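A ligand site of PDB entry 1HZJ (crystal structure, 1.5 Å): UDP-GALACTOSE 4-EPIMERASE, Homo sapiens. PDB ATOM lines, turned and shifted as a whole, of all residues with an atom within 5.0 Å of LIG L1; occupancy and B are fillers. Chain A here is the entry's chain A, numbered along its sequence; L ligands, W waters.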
ATOM      1  N   VAL A  94      18.239   8.886 -13.299  1.00  0.00           N
ATOM      2  CA  VAL A  94      17.464   9.364 -14.442  1.00  0.00           C
ATOM      3  C   VAL A  94      18.244  10.185 -15.469  1.00  0.00           C
ATOM      4  O   VAL A  94      18.234   9.885 -16.681  1.00  0.00           O
ATOM      5  CB  VAL A  94      16.146   9.975 -13.974  1.00  0.00           C
ATOM      6  CG1 VAL A  94      15.273  10.267 -15.176  1.00  0.00           C
ATOM      7  CG2 VAL A  94      15.447   8.975 -13.059  1.00  0.00           C
ATOM      8  N   SER A 132       8.833   0.705  -9.750  1.00  0.00           N
ATOM      9  CA  SER A 132       8.681   2.059  -9.276  1.00  0.00           C
ATOM     10  C   SER A 132       7.446   2.708  -9.840  1.00  0.00           C
ATOM     11  O   SER A 132       7.010   2.418 -10.952  1.00  0.00           O
ATOM     12  CB  SER A 132       9.918   2.770  -9.855  1.00  0.00           C
ATOM     13  OG  SER A 132       9.743   4.175  -9.913  1.00  0.00           O
ATOM     14  N   THR A 134       7.316   5.211 -11.266  1.00  0.00           N
ATOM     15  CA  THR A 134       7.669   5.862 -12.514  1.00  0.00           C
ATOM     16  C   THR A 134       7.014   5.137 -13.732  1.00  0.00           C
ATOM     17  O   THR A 134       6.744   5.752 -14.772  1.00  0.00           O
ATOM     18  CB  THR A 134       9.185   6.026 -12.674  1.00  0.00           C
ATOM     19  OG1 THR A 134       9.506   6.876 -13.741  1.00  0.00           O
ATOM     20  CG2 THR A 134       9.848   4.697 -12.898  1.00  0.00           C
ATOM     21  N   TYR A 157      15.585   5.167 -17.977  1.00  0.00           N
ATOM     22  CA  TYR A 157      15.477   4.485 -16.687  1.00  0.00           C
ATOM     23  C   TYR A 157      14.080   3.904 -16.460  1.00  0.00           C
ATOM     24  O   TYR A 157      13.916   2.716 -16.199  1.00  0.00           O
ATOM     25  CB  TYR A 157      15.828   5.402 -15.496  1.00  0.00           C
ATOM     26  CG  TYR A 157      15.420   4.794 -14.151  1.00  0.00           C
ATOM     27  CD1 TYR A 157      14.371   5.358 -13.406  1.00  0.00           C
ATOM     28  CD2 TYR A 157      16.057   3.662 -13.652  1.00  0.00           C
ATOM     29  CE1 TYR A 157      13.996   4.799 -12.178  1.00  0.00           C
ATOM     30  CE2 TYR A 157      15.696   3.101 -12.420  1.00  0.00           C
ATOM     31  CZ  TYR A 157      14.650   3.669 -11.683  1.00  0.00           C
ATOM     32  OH  TYR A 157      14.276   3.139 -10.463  1.00  0.00           O
ATOM     33  N   PHE A 186       7.107   4.116  -4.209  1.00  0.00           N
ATOM     34  CA  PHE A 186       6.847   5.514  -4.443  1.00  0.00           C
ATOM     35  C   PHE A 186       8.158   6.281  -4.114  1.00  0.00           C
ATOM     36  O   PHE A 186       9.136   6.050  -4.804  1.00  0.00           O
ATOM     37  CB  PHE A 186       5.576   6.058  -3.794  1.00  0.00           C
ATOM     38  CG  PHE A 186       4.415   5.711  -4.719  1.00  0.00           C
ATOM     39  CD1 PHE A 186       3.738   6.693  -5.429  1.00  0.00           C
ATOM     40  CD2 PHE A 186       4.040   4.380  -4.899  1.00  0.00           C
ATOM     41  CE1 PHE A 186       2.692   6.361  -6.307  1.00  0.00           C
ATOM     42  CE2 PHE A 186       3.010   4.021  -5.773  1.00  0.00           C
ATOM     43  CZ  PHE A 186       2.347   5.029  -6.486  1.00  0.00           C
ATOM     44  N   ASN A 187       8.226   7.146  -3.078  1.00  0.00           N
ATOM     45  CA  ASN A 187       9.471   7.883  -2.770  1.00  0.00           C
ATOM     46  C   ASN A 187      10.079   7.455  -1.440  1.00  0.00           C
ATOM     47  O   ASN A 187       9.728   7.955  -0.374  1.00  0.00           O
ATOM     48  CB  ASN A 187       9.186   9.386  -2.785  1.00  0.00           C
ATOM     49  CG  ASN A 187       8.871   9.908  -4.167  1.00  0.00           C
ATOM     50  OD1 ASN A 187       7.873   9.505  -4.756  1.00  0.00           O
ATOM     51  ND2 ASN A 187       9.699  10.790  -4.722  1.00  0.00           N
ATOM     52  N   PRO A 188      10.976   6.501  -1.525  1.00  0.00           N
ATOM     53  CA  PRO A 188      11.637   5.956  -0.347  1.00  0.00           C
ATOM     54  C   PRO A 188      12.462   7.008   0.367  1.00  0.00           C
ATOM     55  O   PRO A 188      13.254   7.775  -0.256  1.00  0.00           O
ATOM     56  CB  PRO A 188      12.509   4.815  -0.840  1.00  0.00           C
ATOM     57  CG  PRO A 188      12.055   4.505  -2.266  1.00  0.00           C
ATOM     58  CD  PRO A 188      11.393   5.778  -2.772  1.00  0.00           C
ATOM     59  N   ASN A 206      20.290  13.348  -6.270  1.00  0.00           N
ATOM     60  CA  ASN A 206      19.269  13.751  -7.220  1.00  0.00           C
ATOM     61  C   ASN A 206      17.880  13.839  -6.582  1.00  0.00           C
ATOM     62  O   ASN A 206      16.974  14.518  -7.095  1.00  0.00           O
ATOM     63  CB  ASN A 206      19.263  12.761  -8.396  1.00  0.00           C
ATOM     64  CG  ASN A 206      20.585  12.770  -9.095  1.00  0.00           C
ATOM     65  OD1 ASN A 206      20.987  13.818  -9.599  1.00  0.00           O
ATOM     66  ND2 ASN A 206      21.219  11.603  -9.145  1.00  0.00           N
ATOM     67  N   ASN A 207      17.709  13.141  -5.452  1.00  0.00           N
ATOM     68  CA  ASN A 207      16.448  13.147  -4.766  1.00  0.00           C
ATOM     69  C   ASN A 207      16.383  14.291  -3.768  1.00  0.00           C
ATOM     70  O   ASN A 207      17.382  14.731  -3.231  1.00  0.00           O
ATOM     71  CB  ASN A 207      16.247  11.825  -4.044  1.00  0.00           C
ATOM     72  CG  ASN A 207      15.994  10.686  -4.995  1.00  0.00           C
ATOM     73  OD1 ASN A 207      16.805   9.779  -5.091  1.00  0.00           O
ATOM     74  ND2 ASN A 207      14.833  10.686  -5.641  1.00  0.00           N
ATOM     75  N   LEU A 208      15.159  14.736  -3.510  1.00  0.00           N
ATOM     76  CA  LEU A 208      14.889  15.834  -2.603  1.00  0.00           C
ATOM     77  C   LEU A 208      15.401  15.695  -1.168  1.00  0.00           C
ATOM     78  O   LEU A 208      16.075  16.564  -0.647  1.00  0.00           O
ATOM     79  CB  LEU A 208      13.360  16.096  -2.556  1.00  0.00           C
ATOM     80  CG  LEU A 208      12.971  17.163  -1.536  1.00  0.00           C
ATOM     81  CD1 LEU A 208      13.390  18.546  -2.018  1.00  0.00           C
ATOM     82  CD2 LEU A 208      11.473  17.138  -1.290  1.00  0.00           C
ATOM     83  N   TYR A 211      19.035  15.881  -0.383  1.00  0.00           N
ATOM     84  CA  TYR A 211      19.504  17.231  -0.629  1.00  0.00           C
ATOM     85  C   TYR A 211      19.121  18.073   0.564  1.00  0.00           C
ATOM     86  O   TYR A 211      19.938  18.844   1.057  1.00  0.00           O
ATOM     87  CB  TYR A 211      18.941  17.841  -1.923  1.00  0.00           C
ATOM     88  CG  TYR A 211      19.849  18.894  -2.508  1.00  0.00           C
ATOM     89  CD1 TYR A 211      19.884  20.172  -1.955  1.00  0.00           C
ATOM     90  CD2 TYR A 211      20.654  18.602  -3.614  1.00  0.00           C
ATOM     91  CE1 TYR A 211      20.749  21.138  -2.485  1.00  0.00           C
ATOM     92  CE2 TYR A 211      21.510  19.562  -4.162  1.00  0.00           C
ATOM     93  CZ  TYR A 211      21.554  20.830  -3.575  1.00  0.00           C
ATOM     94  OH  TYR A 211      22.372  21.793  -4.102  1.00  0.00           O
ATOM     95  N   LEU A 223      18.469  24.815  -0.740  1.00  0.00           N
ATOM     96  CA  LEU A 223      17.756  23.911  -1.592  1.00  0.00           C
ATOM     97  C   LEU A 223      17.239  24.623  -2.835  1.00  0.00           C
ATOM     98  O   LEU A 223      16.613  25.660  -2.768  1.00  0.00           O
ATOM     99  CB  LEU A 223      16.536  23.285  -0.859  1.00  0.00           C
ATOM    100  CG  LEU A 223      15.632  22.440  -1.788  1.00  0.00           C
ATOM    101  CD1 LEU A 223      16.351  21.166  -2.214  1.00  0.00           C
ATOM    102  CD2 LEU A 223      14.314  22.138  -1.102  1.00  0.00           C
ATOM    103  N   ASN A 224      17.471  24.029  -3.981  1.00  0.00           N
ATOM    104  CA  ASN A 224      16.922  24.596  -5.183  1.00  0.00           C
ATOM    105  C   ASN A 224      15.591  23.890  -5.401  1.00  0.00           C
ATOM    106  O   ASN A 224      15.560  22.672  -5.551  1.00  0.00           O
ATOM    107  CB  ASN A 224      17.783  24.295  -6.416  1.00  0.00           C
ATOM    108  CG  ASN A 224      19.179  24.853  -6.251  1.00  0.00           C
ATOM    109  OD1 ASN A 224      20.184  24.134  -6.366  1.00  0.00           O
ATOM    110  ND2 ASN A 224      19.219  26.114  -5.902  1.00  0.00           N
ATOM    111  N   VAL A 225      14.529  24.663  -5.355  1.00  0.00           N
ATOM    112  CA  VAL A 225      13.214  24.127  -5.545  1.00  0.00           C
ATOM    113  C   VAL A 225      12.878  24.189  -7.031  1.00  0.00           C
ATOM    114  O   VAL A 225      12.833  25.271  -7.627  1.00  0.00           O
ATOM    115  CB  VAL A 225      12.204  24.857  -4.691  1.00  0.00           C
ATOM    116  CG1 VAL A 225      10.798  24.461  -5.076  1.00  0.00           C
ATOM    117  CG2 VAL A 225      12.463  24.551  -3.203  1.00  0.00           C
ATOM    118  N   PHE A 226      12.702  23.021  -7.621  1.00  0.00           N
ATOM    119  CA  PHE A 226      12.396  22.869  -9.041  1.00  0.00           C
ATOM    120  C   PHE A 226      10.930  23.268  -9.417  1.00  0.00           C
ATOM    121  O   PHE A 226      10.019  22.462  -9.628  1.00  0.00           O
ATOM    122  CB  PHE A 226      12.730  21.427  -9.473  1.00  0.00           C
ATOM    123  CG  PHE A 226      14.147  20.956  -9.171  1.00  0.00           C
ATOM    124  CD1 PHE A 226      14.402  19.598  -8.966  1.00  0.00           C
ATOM    125  CD2 PHE A 226      15.228  21.848  -9.144  1.00  0.00           C
ATOM    126  CE1 PHE A 226      15.694  19.143  -8.710  1.00  0.00           C
ATOM    127  CE2 PHE A 226      16.533  21.407  -8.899  1.00  0.00           C
ATOM    128  CZ  PHE A 226      16.755  20.058  -8.679  1.00  0.00           C
ATOM    129  N   GLY A 237       5.939  20.570  -6.152  1.00  0.00           N
ATOM    130  CA  GLY A 237       5.592  19.180  -6.401  1.00  0.00           C
ATOM    131  C   GLY A 237       5.171  18.418  -5.171  1.00  0.00           C
ATOM    132  O   GLY A 237       5.723  18.628  -4.089  1.00  0.00           O
ATOM    133  N   VAL A 238       4.195  17.509  -5.358  1.00  0.00           N
ATOM    134  CA  VAL A 238       3.691  16.699  -4.290  1.00  0.00           C
ATOM    135  C   VAL A 238       4.016  15.220  -4.537  1.00  0.00           C
ATOM    136  O   VAL A 238       3.801  14.735  -5.648  1.00  0.00           O
ATOM    137  CB  VAL A 238       2.189  16.927  -4.138  1.00  0.00           C
ATOM    138  CG1 VAL A 238       1.622  15.898  -3.158  1.00  0.00           C
ATOM    139  CG2 VAL A 238       1.960  18.341  -3.627  1.00  0.00           C
ATOM    140  N   ARG A 239       4.559  14.515  -3.525  1.00  0.00           N
ATOM    141  CA  ARG A 239       4.942  13.114  -3.679  1.00  0.00           C
ATOM    142  C   ARG A 239       4.532  12.324  -2.472  1.00  0.00           C
ATOM    143  O   ARG A 239       4.196  12.883  -1.440  1.00  0.00           O
ATOM    144  CB  ARG A 239       6.452  12.927  -3.877  1.00  0.00           C
ATOM    145  CG  ARG A 239       6.939  13.731  -5.079  1.00  0.00           C
ATOM    146  CD  ARG A 239       6.479  13.132  -6.423  1.00  0.00           C
ATOM    147  NE  ARG A 239       7.136  13.793  -7.556  1.00  0.00           N
ATOM    148  CZ  ARG A 239       6.666  14.846  -8.233  1.00  0.00           C
ATOM    149  NH1 ARG A 239       5.494  15.421  -7.904  1.00  0.00           N
ATOM    150  NH2 ARG A 239       7.395  15.352  -9.261  1.00  0.00           N
ATOM    151  N   TYR A 241       6.004  10.158   0.101  1.00  0.00           N
ATOM    152  CA  TYR A 241       7.241   9.744   0.722  1.00  0.00           C
ATOM    153  C   TYR A 241       6.943   8.588   1.642  1.00  0.00           C
ATOM    154  O   TYR A 241       6.007   8.652   2.428  1.00  0.00           O
ATOM    155  CB  TYR A 241       7.927  10.911   1.463  1.00  0.00           C
ATOM    156  CG  TYR A 241       8.261  12.014   0.494  1.00  0.00           C
ATOM    157  CD1 TYR A 241       9.449  11.961  -0.224  1.00  0.00           C
ATOM    158  CD2 TYR A 241       7.353  13.064   0.260  1.00  0.00           C
ATOM    159  CE1 TYR A 241       9.725  12.942  -1.177  1.00  0.00           C
ATOM    160  CE2 TYR A 241       7.632  14.057  -0.672  1.00  0.00           C
ATOM    161  CZ  TYR A 241       8.823  13.967  -1.398  1.00  0.00           C
ATOM    162  OH  TYR A 241       9.119  14.909  -2.338  1.00  0.00           O
ATOM    163  N   VAL A 277       7.055  19.880  -1.558  1.00  0.00           N
ATOM    164  CA  VAL A 277       8.453  20.142  -1.311  1.00  0.00           C
ATOM    165  C   VAL A 277       8.598  21.026  -0.046  1.00  0.00           C
ATOM    166  O   VAL A 277       9.399  20.732   0.854  1.00  0.00           O
ATOM    167  CB  VAL A 277       9.092  20.838  -2.507  1.00  0.00           C
ATOM    168  CG1 VAL A 277      10.539  21.176  -2.208  1.00  0.00           C
ATOM    169  CG2 VAL A 277       9.097  19.915  -3.702  1.00  0.00           C
ATOM    170  N   ARG A 300      12.127  21.148 -13.336  1.00  0.00           N
ATOM    171  CA  ARG A 300      13.003  20.112 -13.782  1.00  0.00           C
ATOM    172  C   ARG A 300      12.272  19.398 -14.905  1.00  0.00           C
ATOM    173  O   ARG A 300      11.067  19.133 -14.823  1.00  0.00           O
ATOM    174  CB  ARG A 300      13.423  19.170 -12.649  1.00  0.00           C
ATOM    175  CG  ARG A 300      14.422  18.112 -13.114  1.00  0.00           C
ATOM    176  CD  ARG A 300      15.017  17.348 -11.952  1.00  0.00           C
ATOM    177  NE  ARG A 300      13.985  16.717 -11.151  1.00  0.00           N
ATOM    178  CZ  ARG A 300      14.205  15.993 -10.046  1.00  0.00           C
ATOM    179  NH1 ARG A 300      15.440  15.771  -9.539  1.00  0.00           N
ATOM    180  NH2 ARG A 300      13.124  15.486  -9.456  1.00  0.00           N
ATOM    181  N   GLU A 301      12.993  19.133 -15.971  1.00  0.00           N
ATOM    182  CA  GLU A 301      12.464  18.457 -17.131  1.00  0.00           C
ATOM    183  C   GLU A 301      11.919  17.078 -16.701  1.00  0.00           C
ATOM    184  O   GLU A 301      12.564  16.315 -15.934  1.00  0.00           O
ATOM    185  CB  GLU A 301      13.612  18.324 -18.157  1.00  0.00           C
ATOM    186  CG  GLU A 301      13.195  18.038 -19.614  1.00  0.00           C
ATOM    187  CD  GLU A 301      14.350  17.500 -20.433  1.00  0.00           C
ATOM    188  OE1 GLU A 301      15.240  18.218 -20.880  1.00  0.00           O
ATOM    189  OE2 GLU A 301      14.278  16.206 -20.593  1.00  0.00           O
ATOM    190  N   ASP A 303       9.350  16.483 -14.671  1.00  0.00           N
ATOM    191  CA  ASP A 303       8.631  16.474 -13.401  1.00  0.00           C
ATOM    192  C   ASP A 303       7.125  16.672 -13.501  1.00  0.00           C
ATOM    193  O   ASP A 303       6.592  17.375 -14.363  1.00  0.00           O
ATOM    194  CB  ASP A 303       9.177  17.510 -12.365  1.00  0.00           C
ATOM    195  CG  ASP A 303      10.442  17.107 -11.663  1.00  0.00           C
ATOM    196  OD1 ASP A 303      10.969  16.008 -11.807  1.00  0.00           O
ATOM    197  OD2 ASP A 303      10.917  18.055 -10.891  1.00  0.00           O
ATOM    198  N   VAL A 304       6.404  16.097 -12.581  1.00  0.00           N
ATOM    199  CA  VAL A 304       4.967  16.304 -12.609  1.00  0.00           C
ATOM    200  C   VAL A 304       4.517  17.023 -11.355  1.00  0.00           C
ATOM    201  O   VAL A 304       5.271  17.134 -10.385  1.00  0.00           O
ATOM    202  CB  VAL A 304       4.196  14.997 -12.792  1.00  0.00           C
ATOM    203  CG1 VAL A 304       4.456  14.385 -14.168  1.00  0.00           C
ATOM    204  CG2 VAL A 304       4.566  13.991 -11.703  1.00  0.00           C
HETATM  205  C1  LIG L   1      12.432  10.930  -8.966  1.00  0.00           C
HETATM  206  C2  LIG L   1      12.844  10.268 -10.279  1.00  0.00           C
HETATM  207  C3  LIG L   1      12.132   8.919 -10.458  1.00  0.00           C
HETATM  208  C4  LIG L   1      12.334   8.024  -9.236  1.00  0.00           C
HETATM  209  C5  LIG L   1      11.851   8.756  -7.989  1.00  0.00           C
HETATM  210  C6  LIG L   1      12.294   8.043  -6.730  1.00  0.00           C
HETATM  211  C7  LIG L   1      13.318  12.093 -11.779  1.00  0.00           C
HETATM  212  C8  LIG L   1      13.025  12.943 -12.980  1.00  0.00           C
HETATM  213  N1  LIG L   1      12.467  11.103 -11.440  1.00  0.00           N
HETATM  214  O1  LIG L   1      11.093  11.342  -9.058  1.00  0.00           O
HETATM  215  O2  LIG L   1      12.696   8.239 -11.579  1.00  0.00           O
HETATM  216  O3  LIG L   1      11.691   6.742  -9.360  1.00  0.00           O
HETATM  217  O4  LIG L   1      12.554  10.012  -7.877  1.00  0.00           O
HETATM  218  O5  LIG L   1      13.725   7.967  -6.792  1.00  0.00           O
HETATM  219  O6  LIG L   1      14.308  12.314 -11.109  1.00  0.00           O
HETATM  220  N2  LIG L   1      12.909  18.558  -5.924  1.00  0.00           N
HETATM  221  C9  LIG L   1      13.293  19.882  -5.731  1.00  0.00           C
HETATM  222  N3  LIG L   1      14.635  20.038  -5.556  1.00  0.00           N
HETATM  223  C10 LIG L   1      15.609  19.029  -5.539  1.00  0.00           C
HETATM  224  C11 LIG L   1      15.088  17.708  -5.754  1.00  0.00           C
HETATM  225  C12 LIG L   1      13.817  17.523  -5.950  1.00  0.00           C
HETATM  226  O7  LIG L   1      12.500  20.816  -5.698  1.00  0.00           O
HETATM  227  O8  LIG L   1      16.762  19.326  -5.357  1.00  0.00           O
HETATM  228  C13 LIG L   1      11.468  18.266  -6.059  1.00  0.00           C
HETATM  229  C14 LIG L   1      11.068  17.589  -7.334  1.00  0.00           C
HETATM  230  O9  LIG L   1      10.691  18.570  -8.304  1.00  0.00           O
HETATM  231  C15 LIG L   1       9.771  16.870  -6.870  1.00  0.00           C
HETATM  232  C16 LIG L   1      10.113  16.434  -5.454  1.00  0.00           C
HETATM  233  O10 LIG L   1      11.147  17.355  -5.027  1.00  0.00           O
HETATM  234  O11 LIG L   1       8.614  17.704  -6.893  1.00  0.00           O
HETATM  235  C17 LIG L   1      10.638  15.023  -5.269  1.00  0.00           C
HETATM  236  O12 LIG L   1      11.742  14.881  -6.148  1.00  0.00           O
HETATM  237  P1  LIG L   1      12.563  13.555  -6.276  1.00  0.00           P
HETATM  238  O13 LIG L   1      13.611  13.648  -7.331  1.00  0.00           O
HETATM  239  O14 LIG L   1      13.142  13.111  -5.005  1.00  0.00           O
HETATM  240  O15 LIG L   1      11.433  12.437  -6.684  1.00  0.00           O
HETATM  241  P2  LIG L   1      10.500  12.335  -7.948  1.00  0.00           P
HETATM  242  O16 LIG L   1       9.212  11.827  -7.400  1.00  0.00           O
HETATM  243  O17 LIG L   1      10.248  13.704  -8.538  1.00  0.00           O
HETATM  244  P1  LG2 L   2      21.055   1.663  -4.826  1.00  0.00           P
HETATM  245  O1  LG2 L   2      21.470   2.153  -3.477  1.00  0.00           O
HETATM  246  O2  LG2 L   2      21.902   2.150  -5.923  1.00  0.00           O
HETATM  247  O3  LG2 L   2      21.137   0.102  -4.736  1.00  0.00           O
HETATM  248  C1  LG2 L   2      21.313  -0.713  -5.907  1.00  0.00           C
HETATM  249  C2  LG2 L   2      22.429  -1.650  -5.641  1.00  0.00           C
HETATM  250  O4  LG2 L   2      22.691  -2.392  -6.868  1.00  0.00           O
HETATM  251  C3  LG2 L   2      23.747  -0.904  -5.320  1.00  0.00           C
HETATM  252  O5  LG2 L   2      24.280  -1.370  -4.081  1.00  0.00           O
HETATM  253  C4  LG2 L   2      24.609  -1.230  -6.567  1.00  0.00           C
HETATM  254  O6  LG2 L   2      26.032  -1.306  -6.337  1.00  0.00           O
HETATM  255  C5  LG2 L   2      24.063  -2.576  -7.014  1.00  0.00           C
HETATM  256  N1  LG2 L   2      24.299  -2.824  -8.433  1.00  0.00           N
HETATM  257  C6  LG2 L   2      24.177  -1.964  -9.505  1.00  0.00           C
HETATM  258  N2  LG2 L   2      24.450  -2.557 -10.682  1.00  0.00           N
HETATM  259  C7  LG2 L   2      24.738  -3.869 -10.326  1.00  0.00           C
HETATM  260  C8  LG2 L   2      25.088  -4.998 -11.104  1.00  0.00           C
HETATM  261  N3  LG2 L   2      25.238  -4.998 -12.447  1.00  0.00           N
HETATM  262  N4  LG2 L   2      25.317  -6.142 -10.437  1.00  0.00           N
HETATM  263  C9  LG2 L   2      25.208  -6.178  -9.058  1.00  0.00           C
HETATM  264  N5  LG2 L   2      24.906  -5.200  -8.257  1.00  0.00           N
HETATM  265  C10 LG2 L   2      24.684  -4.058  -8.947  1.00  0.00           C
HETATM  266  O7  LG2 L   2      19.580   2.066  -5.106  1.00  0.00           O
HETATM  267  P2  LG2 L   2      18.238   1.940  -4.211  1.00  0.00           P
HETATM  268  O8  LG2 L   2      17.723   3.263  -3.888  1.00  0.00           O
HETATM  269  O9  LG2 L   2      18.542   0.991  -3.095  1.00  0.00           O
HETATM  270  O10 LG2 L   2      17.195   1.212  -5.221  1.00  0.00           O
HETATM  271  C11 LG2 L   2      17.035  -0.223  -5.155  1.00  0.00           C
HETATM  272  C12 LG2 L   2      16.222  -0.590  -6.379  1.00  0.00           C
HETATM  273  O11 LG2 L   2      14.962   0.072  -6.236  1.00  0.00           O
HETATM  274  C13 LG2 L   2      16.769  -0.199  -7.784  1.00  0.00           C
HETATM  275  O12 LG2 L   2      16.508  -1.215  -8.781  1.00  0.00           O
HETATM  276  C14 LG2 L   2      15.971   1.078  -8.065  1.00  0.00           C
HETATM  277  O13 LG2 L   2      15.896   1.255  -9.494  1.00  0.00           O
HETATM  278  C15 LG2 L   2      14.634   0.791  -7.404  1.00  0.00           C
HETATM  279  N6  LG2 L   2      13.845   1.986  -7.040  1.00  0.00           N
HETATM  280  C16 LG2 L   2      14.462   2.890  -6.218  1.00  0.00           C
HETATM  281  C17 LG2 L   2      13.843   4.102  -5.941  1.00  0.00           C
HETATM  282  C18 LG2 L   2      14.515   5.128  -4.990  1.00  0.00           C
HETATM  283  O14 LG2 L   2      13.994   6.224  -4.796  1.00  0.00           O
HETATM  284  N7  LG2 L   2      15.642   4.811  -4.326  1.00  0.00           N
HETATM  285  C19 LG2 L   2      12.490   4.355  -6.373  1.00  0.00           C
HETATM  286  C20 LG2 L   2      11.939   3.291  -7.096  1.00  0.00           C
HETATM  287  C21 LG2 L   2      12.528   2.124  -7.483  1.00  0.00           C
HETATM  288  O   HOH W   1      15.610  12.150  -8.911  1.00  0.00           O
HETATM  289  O   HOH W   2       9.496   5.617  -7.495  1.00  0.00           O
HETATM  290  O   HOH W   3      17.196   7.649  -6.541  1.00  0.00           O
HETATM  291  O   HOH W   4      18.794  17.552  -6.804  1.00  0.00           O
HETATM  292  O   HOH W   5       7.380  18.671  -9.168  1.00  0.00           O
HETATM  293  O   HOH W   6      11.986   8.163 -14.116  1.00  0.00           O
HETATM  294  O   HOH W   7      18.339  21.356  -4.786  1.00  0.00           O
HETATM  295  O   HOH W   8      12.228  11.087  -3.454  1.00  0.00           O
HETATM  296  O   HOH W   9      15.767   6.833  -8.971  1.00  0.00           O
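OH of Tyr 157 lies within hydrogen-bond range of O13 of LG2 L2, 2.7 Å away. The guanidinium group (NH2) of Arg 300 is in salt-bridge range of an oxygen (O13) of LIG L1, 2.9 Å away. O9 of LIG L1 sits at hydrogen-bond distance from OD2 of Asp 303, 2.6 Å away. The backbone carbonyl oxygen (O) of Asn 224 sits at hydrogen-bond distance from a nitrogen (N3) of LIG L1 (2.8 Å). N of Phe 226 is in hydrogen-bond range of O7 of LIG L1 (2.9 Å). N of Leu 208 sits at hydrogen-bond distance from O14 of LIG L1. The side-chain amide nitrogen (ND2) of Asn 207 lies within hydrogen-bond range of an oxygen (O14) of LIG L1 (3.0 Å). The side-chain amide nitrogen (ND2) of Asn 187 is in hydrogen-bond range of an oxygen (O16) of LIG L1. An oxygen (O3) of LIG L1 lies within hydrogen-bond range of the side-chain hydroxyl (OG) of Ser 132, at 3.3 Å. The guanidinium group (NE) of Arg 239 is in salt-bridge range of an oxygen (O16) of LIG L1 (2.9 Å).
An oxygen (O5) of LIG L1 sits at hydrogen-bond distance from an oxygen (O14) of LG2 L2 (2.7 Å).
The guanidinium group (NH2) of Arg 239 is in hydrogen-bond range of the backbone carbonyl oxygen (O) of Val 304, at 3.0 Å. NH1 of Arg 300 sits at hydrogen-bond distance from O of Asn 206 (3.1 Å). The backbone carbonyl oxygen of Gly 237 is in hydrogen-bond range of the backbone NH of Val 277 (3.1 Å). The side-chain carboxylate (OD1) of Asp 303 is in salt-bridge range of the guanidinium group (NE) of Arg 300, at 3.2 Å. The backbone NH of Thr 134 sits close to the side-chain hydroxyl of Ser 132.
O of Asn 206 lies close to O13 of LIG L1 (3.5 Å). Val 94 touches LIG L1. Tyr 157 touches LIG L1 (CE1 to O2, 3.7 Å). CD1 of Leu 223 touches O8 of LIG L1, at 3.7 Å. Val 225 touches LIG L1 (CA to O7, 3.4 Å). Gly 237 touches LIG L1. Tyr 241 touches LIG L1 (OH to C17, 3.3 Å). Val 277 touches LIG L1. Hydrophobic or aromatic side chains within 4 Å of LIG L1: Val 94, Tyr 157, Leu 208, Leu 223, Phe 226 and Val 277. 17 residues have an atom within 4 Å of LIG L1: Val 94, Ser 132, Tyr 157, Asn 187, Asn 206, Asn 207, Leu 208, Leu 223, Asn 224, Val 225, Phe 226, Gly 237, Arg 239, Tyr 241, Val 277, Arg 300 and Asp 303.
Water W7 lies within hydrogen-bond range of an oxygen (O8) of LIG L1 and the backbone NH of Asn 224. Water W6 bridges O2 of LIG L1 (2.6 Å) and OG1 of Thr 134 (2.8 Å). Water W8 lies within hydrogen-bond range of an oxygen (O14) of LIG L1 (2.7 Å), the side-chain amide nitrogen of Asn 187 (2.8 Å) and the side-chain amide nitrogen of Asn 207 (3.4 Å). Water W5 lies within hydrogen-bond range of O11 of LIG L1, O of Val 304 and NH2 of Arg 239. Water W2 lies within hydrogen-bond range of the backbone carbonyl oxygen of Phe 186, the side-chain hydroxyl of Ser 132 and an oxygen (O3) of LIG L1. Water W3 lies within hydrogen-bond range of the side-chain amide oxygen (OD1) of Asn 207 (2.6 Å) and an oxygen (O5) of LIG L1 (3.5 Å).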
